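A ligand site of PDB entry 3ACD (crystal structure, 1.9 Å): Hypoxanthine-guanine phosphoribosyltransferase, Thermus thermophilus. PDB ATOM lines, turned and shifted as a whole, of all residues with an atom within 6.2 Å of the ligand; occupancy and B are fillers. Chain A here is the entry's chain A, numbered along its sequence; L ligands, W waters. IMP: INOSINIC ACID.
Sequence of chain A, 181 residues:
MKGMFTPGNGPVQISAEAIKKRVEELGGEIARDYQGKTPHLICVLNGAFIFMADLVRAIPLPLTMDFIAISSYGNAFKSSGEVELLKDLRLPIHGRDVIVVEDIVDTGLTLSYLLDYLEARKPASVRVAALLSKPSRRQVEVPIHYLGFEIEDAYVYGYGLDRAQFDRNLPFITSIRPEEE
Water W10 lies within hydrogen-bond range of O3P of the ligand (2.7 Å) and N of Leu 111 (2.9 Å).
Water W8 bridges O3' of the ligand (2.7 Å) and OE2 of Glu 102 (3.4 Å).
Water W7 bridges an oxygen (O1P) of the ligand (2.8 Å) and the side-chain carboxylate of Asp 106 (2.8 Å).
Water W4 lies within hydrogen-bond range of O2' of the ligand (3.0 Å), N of Gly 47 (3.0 Å) and OD2 of Asp 103 (3.3 Å).
Water W5 bridges the side-chain carboxylate (OD2) of Asp 103 (2.9 Å) and a nitrogen (N3) of the ligand (3.1 Å).
Water W6 lies within hydrogen-bond range of NZ of Lys 134, OD2 of Asp 106 and N7 of the ligand.
O3' of the ligand is in hydrogen-bond range of OE1 of Glu 102.
N of Asp 106 lies within hydrogen-bond range of O3P of the ligand, at 2.8 Å.
N of Gly 108 sits at hydrogen-bond distance from O3P of the ligand (2.8 Å).
O3' of the ligand sits at hydrogen-bond distance from OD1 of Asp 103 (2.7 Å).
OG1 of Thr 107 sits at hydrogen-bond distance from O1P of the ligand (2.7 Å).
O6 of the ligand sits at hydrogen-bond distance from NZ of Lys 134, 2.9 Å away.
The backbone NH (N) of Thr 110 is in hydrogen-bond range of an oxygen (O2P) of the ligand (2.8 Å).
N of Thr 107 is in hydrogen-bond range of O1P of the ligand, at 2.8 Å.
O of Val 156 sits at hydrogen-bond distance from N1 of the ligand (2.6 Å).
OG1 of Thr 110 lies within hydrogen-bond range of O2P of the ligand.
An oxygen (O6) of the ligand sits at hydrogen-bond distance from the backbone NH of Val 156, at 3.0 Å.
O6 of the ligand lies close to O of Ala 154 (3.5 Å).
O of Ile 104 touches C3' of the ligand, at 3.3 Å.
Val 105 touches the ligand (C to O3P, 3.8 Å).
Leu 109 touches the ligand.
Tyr 155 touches the ligand (CE1 to N1, 3.4 Å).
Of the 22 residues printed, 13 come within 4 Å of the ligand.
The side-chain hydroxyl (OH) of Tyr 155 sits at hydrogen-bond distance from the backbone carbonyl oxygen (O) of Asp 162.
The guanidinium group (NE) of Arg 138 is in hydrogen-bond range of the backbone carbonyl oxygen (O) of Asp 106, 2.8 Å away.
NZ of Lys 134 is in hydrogen-bond range of O of Ala 154, at 3.3 Å.
The backbone carbonyl oxygen (O) of Lys 134 is in hydrogen-bond range of the guanidinium group (NH2) of Arg 138, at 3.4 Å.
The backbone carbonyl oxygen of Val 105 sits at hydrogen-bond distance from the guanidinium group of Arg 138 (3.1 Å).
N of Leu 109 lies close to OG1 of Thr 107 (3.3 Å).
N of Lys 134 lies within hydrogen-bond range of O of Val 105, at 3.0 Å.
The side-chain carboxylate (OD1) of Asp 106 lies within salt-bridge range of the guanidinium group (NE) of Arg 137 (2.9 Å).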
ATOM      1  N   VAL A  44     -21.356  11.624  -7.823  1.00  0.00           N
ATOM      2  CA  VAL A  44     -22.620  11.838  -7.139  1.00  0.00           C
ATOM      3  C   VAL A  44     -23.746  11.452  -8.092  1.00  0.00           C
ATOM      4  O   VAL A  44     -24.050  12.148  -9.055  1.00  0.00           O
ATOM      5  CB  VAL A  44     -22.794  13.322  -6.715  1.00  0.00           C
ATOM      6  CG1 VAL A  44     -24.159  13.520  -6.063  1.00  0.00           C
ATOM      7  CG2 VAL A  44     -21.694  13.714  -5.736  1.00  0.00           C
ATOM      8  N   GLY A  47     -27.307  12.107 -11.532  1.00  0.00           N
ATOM      9  CA  GLY A  47     -26.935  13.088 -12.530  1.00  0.00           C
ATOM     10  C   GLY A  47     -25.530  13.220 -13.081  1.00  0.00           C
ATOM     11  O   GLY A  47     -25.356  13.606 -14.246  1.00  0.00           O
ATOM     12  N   GLU A 102     -19.656  16.214  -9.459  1.00  0.00           N
ATOM     13  CA  GLU A 102     -21.060  16.627  -9.438  1.00  0.00           C
ATOM     14  C   GLU A 102     -21.580  17.017 -10.815  1.00  0.00           C
ATOM     15  O   GLU A 102     -20.812  17.353 -11.696  1.00  0.00           O
ATOM     16  CB  GLU A 102     -21.224  17.812  -8.495  1.00  0.00           C
ATOM     17  CG  GLU A 102     -21.467  17.424  -7.051  1.00  0.00           C
ATOM     18  CD  GLU A 102     -22.907  17.061  -6.802  1.00  0.00           C
ATOM     19  OE1 GLU A 102     -23.586  16.618  -7.755  1.00  0.00           O
ATOM     20  OE2 GLU A 102     -23.376  17.212  -5.647  1.00  0.00           O
ATOM     21  N   ASP A 103     -22.908  16.989 -10.974  1.00  0.00           N
ATOM     22  CA  ASP A 103     -23.501  17.373 -12.247  1.00  0.00           C
ATOM     23  C   ASP A 103     -23.655  18.889 -12.321  1.00  0.00           C
ATOM     24  O   ASP A 103     -23.096  19.532 -13.215  1.00  0.00           O
ATOM     25  CB  ASP A 103     -24.865  16.682 -12.466  1.00  0.00           C
ATOM     26  CG  ASP A 103     -25.847  16.870 -11.302  1.00  0.00           C
ATOM     27  OD1 ASP A 103     -25.473  17.430 -10.247  1.00  0.00           O
ATOM     28  OD2 ASP A 103     -27.006  16.438 -11.457  1.00  0.00           O
ATOM     29  N   ILE A 104     -24.376  19.462 -11.369  1.00  0.00           N
ATOM     30  CA  ILE A 104     -24.599  20.904 -11.357  1.00  0.00           C
ATOM     31  C   ILE A 104     -24.775  21.420  -9.935  1.00  0.00           C
ATOM     32  O   ILE A 104     -25.467  20.815  -9.120  1.00  0.00           O
ATOM     33  CB  ILE A 104     -25.836  21.275 -12.207  1.00  0.00           C
ATOM     34  CG1 ILE A 104     -26.083  22.783 -12.167  1.00  0.00           C
ATOM     35  CG2 ILE A 104     -27.066  20.530 -11.698  1.00  0.00           C
ATOM     36  CD1 ILE A 104     -27.143  23.230 -13.167  1.00  0.00           C
ATOM     37  N   VAL A 105     -24.123  22.540  -9.632  1.00  0.00           N
ATOM     38  CA  VAL A 105     -24.233  23.154  -8.315  1.00  0.00           C
ATOM     39  C   VAL A 105     -25.258  24.276  -8.458  1.00  0.00           C
ATOM     40  O   VAL A 105     -25.072  25.218  -9.230  1.00  0.00           O
ATOM     41  CB  VAL A 105     -22.871  23.721  -7.841  1.00  0.00           C
ATOM     42  CG1 VAL A 105     -23.017  24.318  -6.438  1.00  0.00           C
ATOM     43  CG2 VAL A 105     -21.831  22.605  -7.839  1.00  0.00           C
ATOM     44  N   ASP A 106     -26.356  24.151  -7.716  1.00  0.00           N
ATOM     45  CA  ASP A 106     -27.440  25.122  -7.755  1.00  0.00           C
ATOM     46  C   ASP A 106     -27.348  26.002  -6.517  1.00  0.00           C
ATOM     47  O   ASP A 106     -26.603  26.974  -6.520  1.00  0.00           O
ATOM     48  CB  ASP A 106     -28.783  24.374  -7.812  1.00  0.00           C
ATOM     49  CG  ASP A 106     -29.978  25.304  -7.990  1.00  0.00           C
ATOM     50  OD1 ASP A 106     -29.783  26.480  -8.362  1.00  0.00           O
ATOM     51  OD2 ASP A 106     -31.110  24.844  -7.768  1.00  0.00           O
ATOM     52  N   THR A 107     -28.083  25.652  -5.459  1.00  0.00           N
ATOM     53  CA  THR A 107     -28.012  26.448  -4.231  1.00  0.00           C
ATOM     54  C   THR A 107     -26.722  26.130  -3.487  1.00  0.00           C
ATOM     55  O   THR A 107     -26.225  26.941  -2.699  1.00  0.00           O
ATOM     56  CB  THR A 107     -29.202  26.156  -3.276  1.00  0.00           C
ATOM     57  OG1 THR A 107     -29.093  24.824  -2.767  1.00  0.00           O
ATOM     58  CG2 THR A 107     -30.527  26.307  -4.007  1.00  0.00           C
ATOM     59  N   GLY A 108     -26.176  24.935  -3.738  1.00  0.00           N
ATOM     60  CA  GLY A 108     -24.954  24.520  -3.092  1.00  0.00           C
ATOM     61  C   GLY A 108     -25.162  23.746  -1.798  1.00  0.00           C
ATOM     62  O   GLY A 108     -24.204  23.245  -1.212  1.00  0.00           O
ATOM     63  N   LEU A 109     -26.405  23.641  -1.349  1.00  0.00           N
ATOM     64  CA  LEU A 109     -26.719  22.933  -0.111  1.00  0.00           C
ATOM     65  C   LEU A 109     -26.251  21.471  -0.126  1.00  0.00           C
ATOM     66  O   LEU A 109     -25.610  21.019   0.818  1.00  0.00           O
ATOM     67  CB  LEU A 109     -28.219  22.995   0.159  1.00  0.00           C
ATOM     68  CG  LEU A 109     -28.784  24.404   0.390  1.00  0.00           C
ATOM     69  CD1 LEU A 109     -30.305  24.342   0.507  1.00  0.00           C
ATOM     70  CD2 LEU A 109     -28.174  24.999   1.646  1.00  0.00           C
ATOM     71  N   THR A 110     -26.570  20.744  -1.185  1.00  0.00           N
ATOM     72  CA  THR A 110     -26.176  19.346  -1.274  1.00  0.00           C
ATOM     73  C   THR A 110     -24.665  19.165  -1.214  1.00  0.00           C
ATOM     74  O   THR A 110     -24.161  18.346  -0.435  1.00  0.00           O
ATOM     75  CB  THR A 110     -26.712  18.682  -2.551  1.00  0.00           C
ATOM     76  OG1 THR A 110     -28.138  18.797  -2.580  1.00  0.00           O
ATOM     77  CG2 THR A 110     -26.343  17.204  -2.576  1.00  0.00           C
ATOM     78  N   LEU A 111     -23.939  19.912  -2.044  1.00  0.00           N
ATOM     79  CA  LEU A 111     -22.490  19.802  -2.054  1.00  0.00           C
ATOM     80  C   LEU A 111     -21.915  20.163  -0.681  1.00  0.00           C
ATOM     81  O   LEU A 111     -20.963  19.548  -0.223  1.00  0.00           O
ATOM     82  CB  LEU A 111     -21.900  20.703  -3.141  1.00  0.00           C
ATOM     83  CG  LEU A 111     -20.367  20.691  -3.290  1.00  0.00           C
ATOM     84  CD1 LEU A 111     -19.881  19.265  -3.507  1.00  0.00           C
ATOM     85  CD2 LEU A 111     -19.970  21.580  -4.466  1.00  0.00           C
ATOM     86  N   LYS A 134     -24.801  27.379 -11.281  1.00  0.00           N
ATOM     87  CA  LYS A 134     -25.734  28.512 -11.409  1.00  0.00           C
ATOM     88  C   LYS A 134     -25.522  29.374 -10.164  1.00  0.00           C
ATOM     89  O   LYS A 134     -26.331  29.366  -9.230  1.00  0.00           O
ATOM     90  CB  LYS A 134     -27.175  27.998 -11.459  1.00  0.00           C
ATOM     91  CG  LYS A 134     -27.476  27.113 -12.671  1.00  0.00           C
ATOM     92  CD  LYS A 134     -28.940  26.680 -12.734  1.00  0.00           C
ATOM     93  CE  LYS A 134     -29.305  25.732 -11.606  1.00  0.00           C
ATOM     94  NZ  LYS A 134     -30.692  25.188 -11.762  1.00  0.00           N
ATOM     95  N   ARG A 137     -27.934  31.434  -7.914  1.00  0.00           N
ATOM     96  CA  ARG A 137     -28.808  30.670  -7.029  1.00  0.00           C
ATOM     97  C   ARG A 137     -28.116  30.230  -5.736  1.00  0.00           C
ATOM     98  O   ARG A 137     -28.753  29.691  -4.830  1.00  0.00           O
ATOM     99  CB  ARG A 137     -29.330  29.434  -7.765  1.00  0.00           C
ATOM    100  CG  ARG A 137     -30.332  29.722  -8.868  1.00  0.00           C
ATOM    101  CD  ARG A 137     -31.752  29.592  -8.334  1.00  0.00           C
ATOM    102  NE  ARG A 137     -32.025  28.220  -7.903  1.00  0.00           N
ATOM    103  CZ  ARG A 137     -33.124  27.828  -7.268  1.00  0.00           C
ATOM    104  NH1 ARG A 137     -34.070  28.713  -6.988  1.00  0.00           N
ATOM    105  NH2 ARG A 137     -33.274  26.563  -6.918  1.00  0.00           N
ATOM    106  N   ARG A 138     -26.811  30.474  -5.654  1.00  0.00           N
ATOM    107  CA  ARG A 138     -25.997  30.062  -4.512  1.00  0.00           C
ATOM    108  C   ARG A 138     -26.477  30.600  -3.160  1.00  0.00           C
ATOM    109  O   ARG A 138     -26.584  31.807  -2.951  1.00  0.00           O
ATOM    110  CB  ARG A 138     -24.538  30.462  -4.759  1.00  0.00           C
ATOM    111  CG  ARG A 138     -23.489  29.675  -3.980  1.00  0.00           C
ATOM    112  CD  ARG A 138     -23.665  28.164  -4.172  1.00  0.00           C
ATOM    113  NE  ARG A 138     -24.066  27.808  -5.539  1.00  0.00           N
ATOM    114  CZ  ARG A 138     -23.275  27.883  -6.603  1.00  0.00           C
ATOM    115  NH1 ARG A 138     -22.020  28.284  -6.483  1.00  0.00           N
ATOM    116  NH2 ARG A 138     -23.766  27.578  -7.803  1.00  0.00           N
ATOM    117  N   ILE A 151     -23.402  29.008 -15.750  1.00  0.00           N
ATOM    118  CA  ILE A 151     -24.587  29.384 -16.513  1.00  0.00           C
ATOM    119  C   ILE A 151     -25.576  30.247 -15.736  1.00  0.00           C
ATOM    120  O   ILE A 151     -25.512  30.371 -14.521  1.00  0.00           O
ATOM    121  CB  ILE A 151     -25.347  28.133 -17.011  1.00  0.00           C
ATOM    122  CG1 ILE A 151     -25.854  27.327 -15.810  1.00  0.00           C
ATOM    123  CG2 ILE A 151     -24.429  27.277 -17.869  1.00  0.00           C
ATOM    124  CD1 ILE A 151     -26.779  26.165 -16.182  1.00  0.00           C
ATOM    125  N   ALA A 154     -31.486  28.688 -14.825  1.00  0.00           N
ATOM    126  CA  ALA A 154     -32.420  27.992 -15.696  1.00  0.00           C
ATOM    127  C   ALA A 154     -32.406  26.501 -15.357  1.00  0.00           C
ATOM    128  O   ALA A 154     -31.403  25.998 -14.845  1.00  0.00           O
ATOM    129  CB  ALA A 154     -32.028  28.191 -17.155  1.00  0.00           C
ATOM    130  N   TYR A 155     -33.507  25.803 -15.617  1.00  0.00           N
ATOM    131  CA  TYR A 155     -33.534  24.373 -15.347  1.00  0.00           C
ATOM    132  C   TYR A 155     -32.981  23.671 -16.568  1.00  0.00           C
ATOM    133  O   TYR A 155     -33.587  23.713 -17.644  1.00  0.00           O
ATOM    134  CB  TYR A 155     -34.948  23.858 -15.089  1.00  0.00           C
ATOM    135  CG  TYR A 155     -34.932  22.421 -14.625  1.00  0.00           C
ATOM    136  CD1 TYR A 155     -34.658  22.101 -13.296  1.00  0.00           C
ATOM    137  CD2 TYR A 155     -35.092  21.369 -15.531  1.00  0.00           C
ATOM    138  CE1 TYR A 155     -34.529  20.787 -12.876  1.00  0.00           C
ATOM    139  CE2 TYR A 155     -34.957  20.036 -15.120  1.00  0.00           C
ATOM    140  CZ  TYR A 155     -34.682  19.753 -13.792  1.00  0.00           C
ATOM    141  OH  TYR A 155     -34.510  18.455 -13.377  1.00  0.00           O
ATOM    142  N   VAL A 156     -31.831  23.035 -16.409  1.00  0.00           N
ATOM    143  CA  VAL A 156     -31.197  22.331 -17.510  1.00  0.00           C
ATOM    144  C   VAL A 156     -31.373  20.826 -17.404  1.00  0.00           C
ATOM    145  O   VAL A 156     -31.699  20.288 -16.344  1.00  0.00           O
ATOM    146  CB  VAL A 156     -29.676  22.652 -17.565  1.00  0.00           C
ATOM    147  CG1 VAL A 156     -29.464  24.150 -17.761  1.00  0.00           C
ATOM    148  CG2 VAL A 156     -29.001  22.188 -16.278  1.00  0.00           C
ATOM    149  N   TYR A 157     -31.158  20.126 -18.517  1.00  0.00           N
ATOM    150  CA  TYR A 157     -31.267  18.683 -18.529  1.00  0.00           C
ATOM    151  C   TYR A 157     -30.481  18.118 -19.701  1.00  0.00           C
ATOM    152  O   TYR A 157     -30.040  18.863 -20.581  1.00  0.00           O
ATOM    153  CB  TYR A 157     -32.736  18.247 -18.564  1.00  0.00           C
ATOM    154  CG  TYR A 157     -33.521  18.717 -19.765  1.00  0.00           C
ATOM    155  CD1 TYR A 157     -33.660  17.907 -20.890  1.00  0.00           C
ATOM    156  CD2 TYR A 157     -34.149  19.968 -19.771  1.00  0.00           C
ATOM    157  CE1 TYR A 157     -34.404  18.326 -21.992  1.00  0.00           C
ATOM    158  CE2 TYR A 157     -34.886  20.393 -20.878  1.00  0.00           C
ATOM    159  CZ  TYR A 157     -35.005  19.571 -21.987  1.00  0.00           C
ATOM    160  OH  TYR A 157     -35.732  20.001 -23.078  1.00  0.00           O
ATOM    161  N   LEU A 161     -28.310  14.678 -16.683  1.00  0.00           N
ATOM    162  CA  LEU A 161     -29.275  15.413 -15.879  1.00  0.00           C
ATOM    163  C   LEU A 161     -30.686  15.136 -16.380  1.00  0.00           C
ATOM    164  O   LEU A 161     -30.932  15.121 -17.584  1.00  0.00           O
ATOM    165  CB  LEU A 161     -28.968  16.914 -15.916  1.00  0.00           C
ATOM    166  CG  LEU A 161     -27.702  17.369 -15.184  1.00  0.00           C
ATOM    167  CD1 LEU A 161     -26.468  16.777 -15.853  1.00  0.00           C
ATOM    168  CD2 LEU A 161     -27.619  18.890 -15.193  1.00  0.00           C
ATOM    169  N   ASP A 162     -31.611  14.934 -15.450  1.00  0.00           N
ATOM    170  CA  ASP A 162     -32.986  14.601 -15.810  1.00  0.00           C
ATOM    171  C   ASP A 162     -34.006  15.715 -15.751  1.00  0.00           C
ATOM    172  O   ASP A 162     -33.786  16.789 -15.173  1.00  0.00           O
ATOM    173  CB  ASP A 162     -33.481  13.475 -14.910  1.00  0.00           C
ATOM    174  CG  ASP A 162     -33.764  13.957 -13.488  1.00  0.00           C
ATOM    175  OD1 ASP A 162     -32.828  14.454 -12.843  1.00  0.00           O
ATOM    176  OD2 ASP A 162     -34.920  13.850 -13.041  1.00  0.00           O
HETATM  177  P   IMP L   1     -28.228  22.089  -4.919  1.00  0.00           P
HETATM  178  O1P IMP L   1     -29.256  23.150  -4.863  1.00  0.00           O
HETATM  179  O2P IMP L   1     -28.115  21.372  -3.481  1.00  0.00           O
HETATM  180  O3P IMP L   1     -26.804  22.750  -5.312  1.00  0.00           O
HETATM  181  O5' IMP L   1     -28.660  21.018  -6.057  1.00  0.00           O
HETATM  182  C5' IMP L   1     -28.315  19.644  -5.874  1.00  0.00           C
HETATM  183  C4' IMP L   1     -28.874  18.790  -7.018  1.00  0.00           C
HETATM  184  O4' IMP L   1     -30.052  19.410  -7.610  1.00  0.00           O
HETATM  185  C3' IMP L   1     -27.860  18.731  -8.193  1.00  0.00           C
HETATM  186  O3' IMP L   1     -26.832  17.772  -7.958  1.00  0.00           O
HETATM  187  C2' IMP L   1     -28.792  18.303  -9.340  1.00  0.00           C
HETATM  188  O2' IMP L   1     -28.969  16.877  -9.366  1.00  0.00           O
HETATM  189  C1' IMP L   1     -30.119  19.009  -9.000  1.00  0.00           C
HETATM  190  N9  IMP L   1     -30.282  20.187  -9.896  1.00  0.00           N
HETATM  191  C8  IMP L   1     -30.108  21.508  -9.561  1.00  0.00           C
HETATM  192  N7  IMP L   1     -30.337  22.270 -10.612  1.00  0.00           N
HETATM  193  C5  IMP L   1     -30.661  21.479 -11.660  1.00  0.00           C
HETATM  194  C6  IMP L   1     -31.016  21.701 -13.031  1.00  0.00           C
HETATM  195  O6  IMP L   1     -31.057  22.835 -13.481  1.00  0.00           O
HETATM  196  N1  IMP L   1     -31.294  20.614 -13.822  1.00  0.00           N
HETATM  197  C2  IMP L   1     -31.244  19.339 -13.321  1.00  0.00           C
HETATM  198  N3  IMP L   1     -30.927  19.111 -12.057  1.00  0.00           N
HETATM  199  C4  IMP L   1     -30.632  20.134 -11.208  1.00  0.00           C
HETATM  200  O   HOH W   1     -30.493  21.413  -2.210  1.00  0.00           O
HETATM  201  O   HOH W   2     -31.228  15.633  -8.670  1.00  0.00           O
HETATM  202  O   HOH W   3     -24.485  19.642  -6.618  1.00  0.00           O
HETATM  203  O   HOH W   4     -27.933  14.090  -9.389  1.00  0.00           O
HETATM  204  O   HOH W   5     -29.706  16.353 -12.554  1.00  0.00           O
HETATM  205  O   HOH W   6     -32.859  24.242 -10.064  1.00  0.00           O
HETATM  206  O   HOH W   7     -31.776  22.847  -5.961  1.00  0.00           O
HETATM  207  O   HOH W   8     -26.490  16.011  -5.955  1.00  0.00           O
HETATM  208  O   HOH W   9     -32.584  20.321  -6.594  1.00  0.00           O
HETATM  209  O   HOH W  10     -24.691  21.350  -4.499  1.00  0.00           O
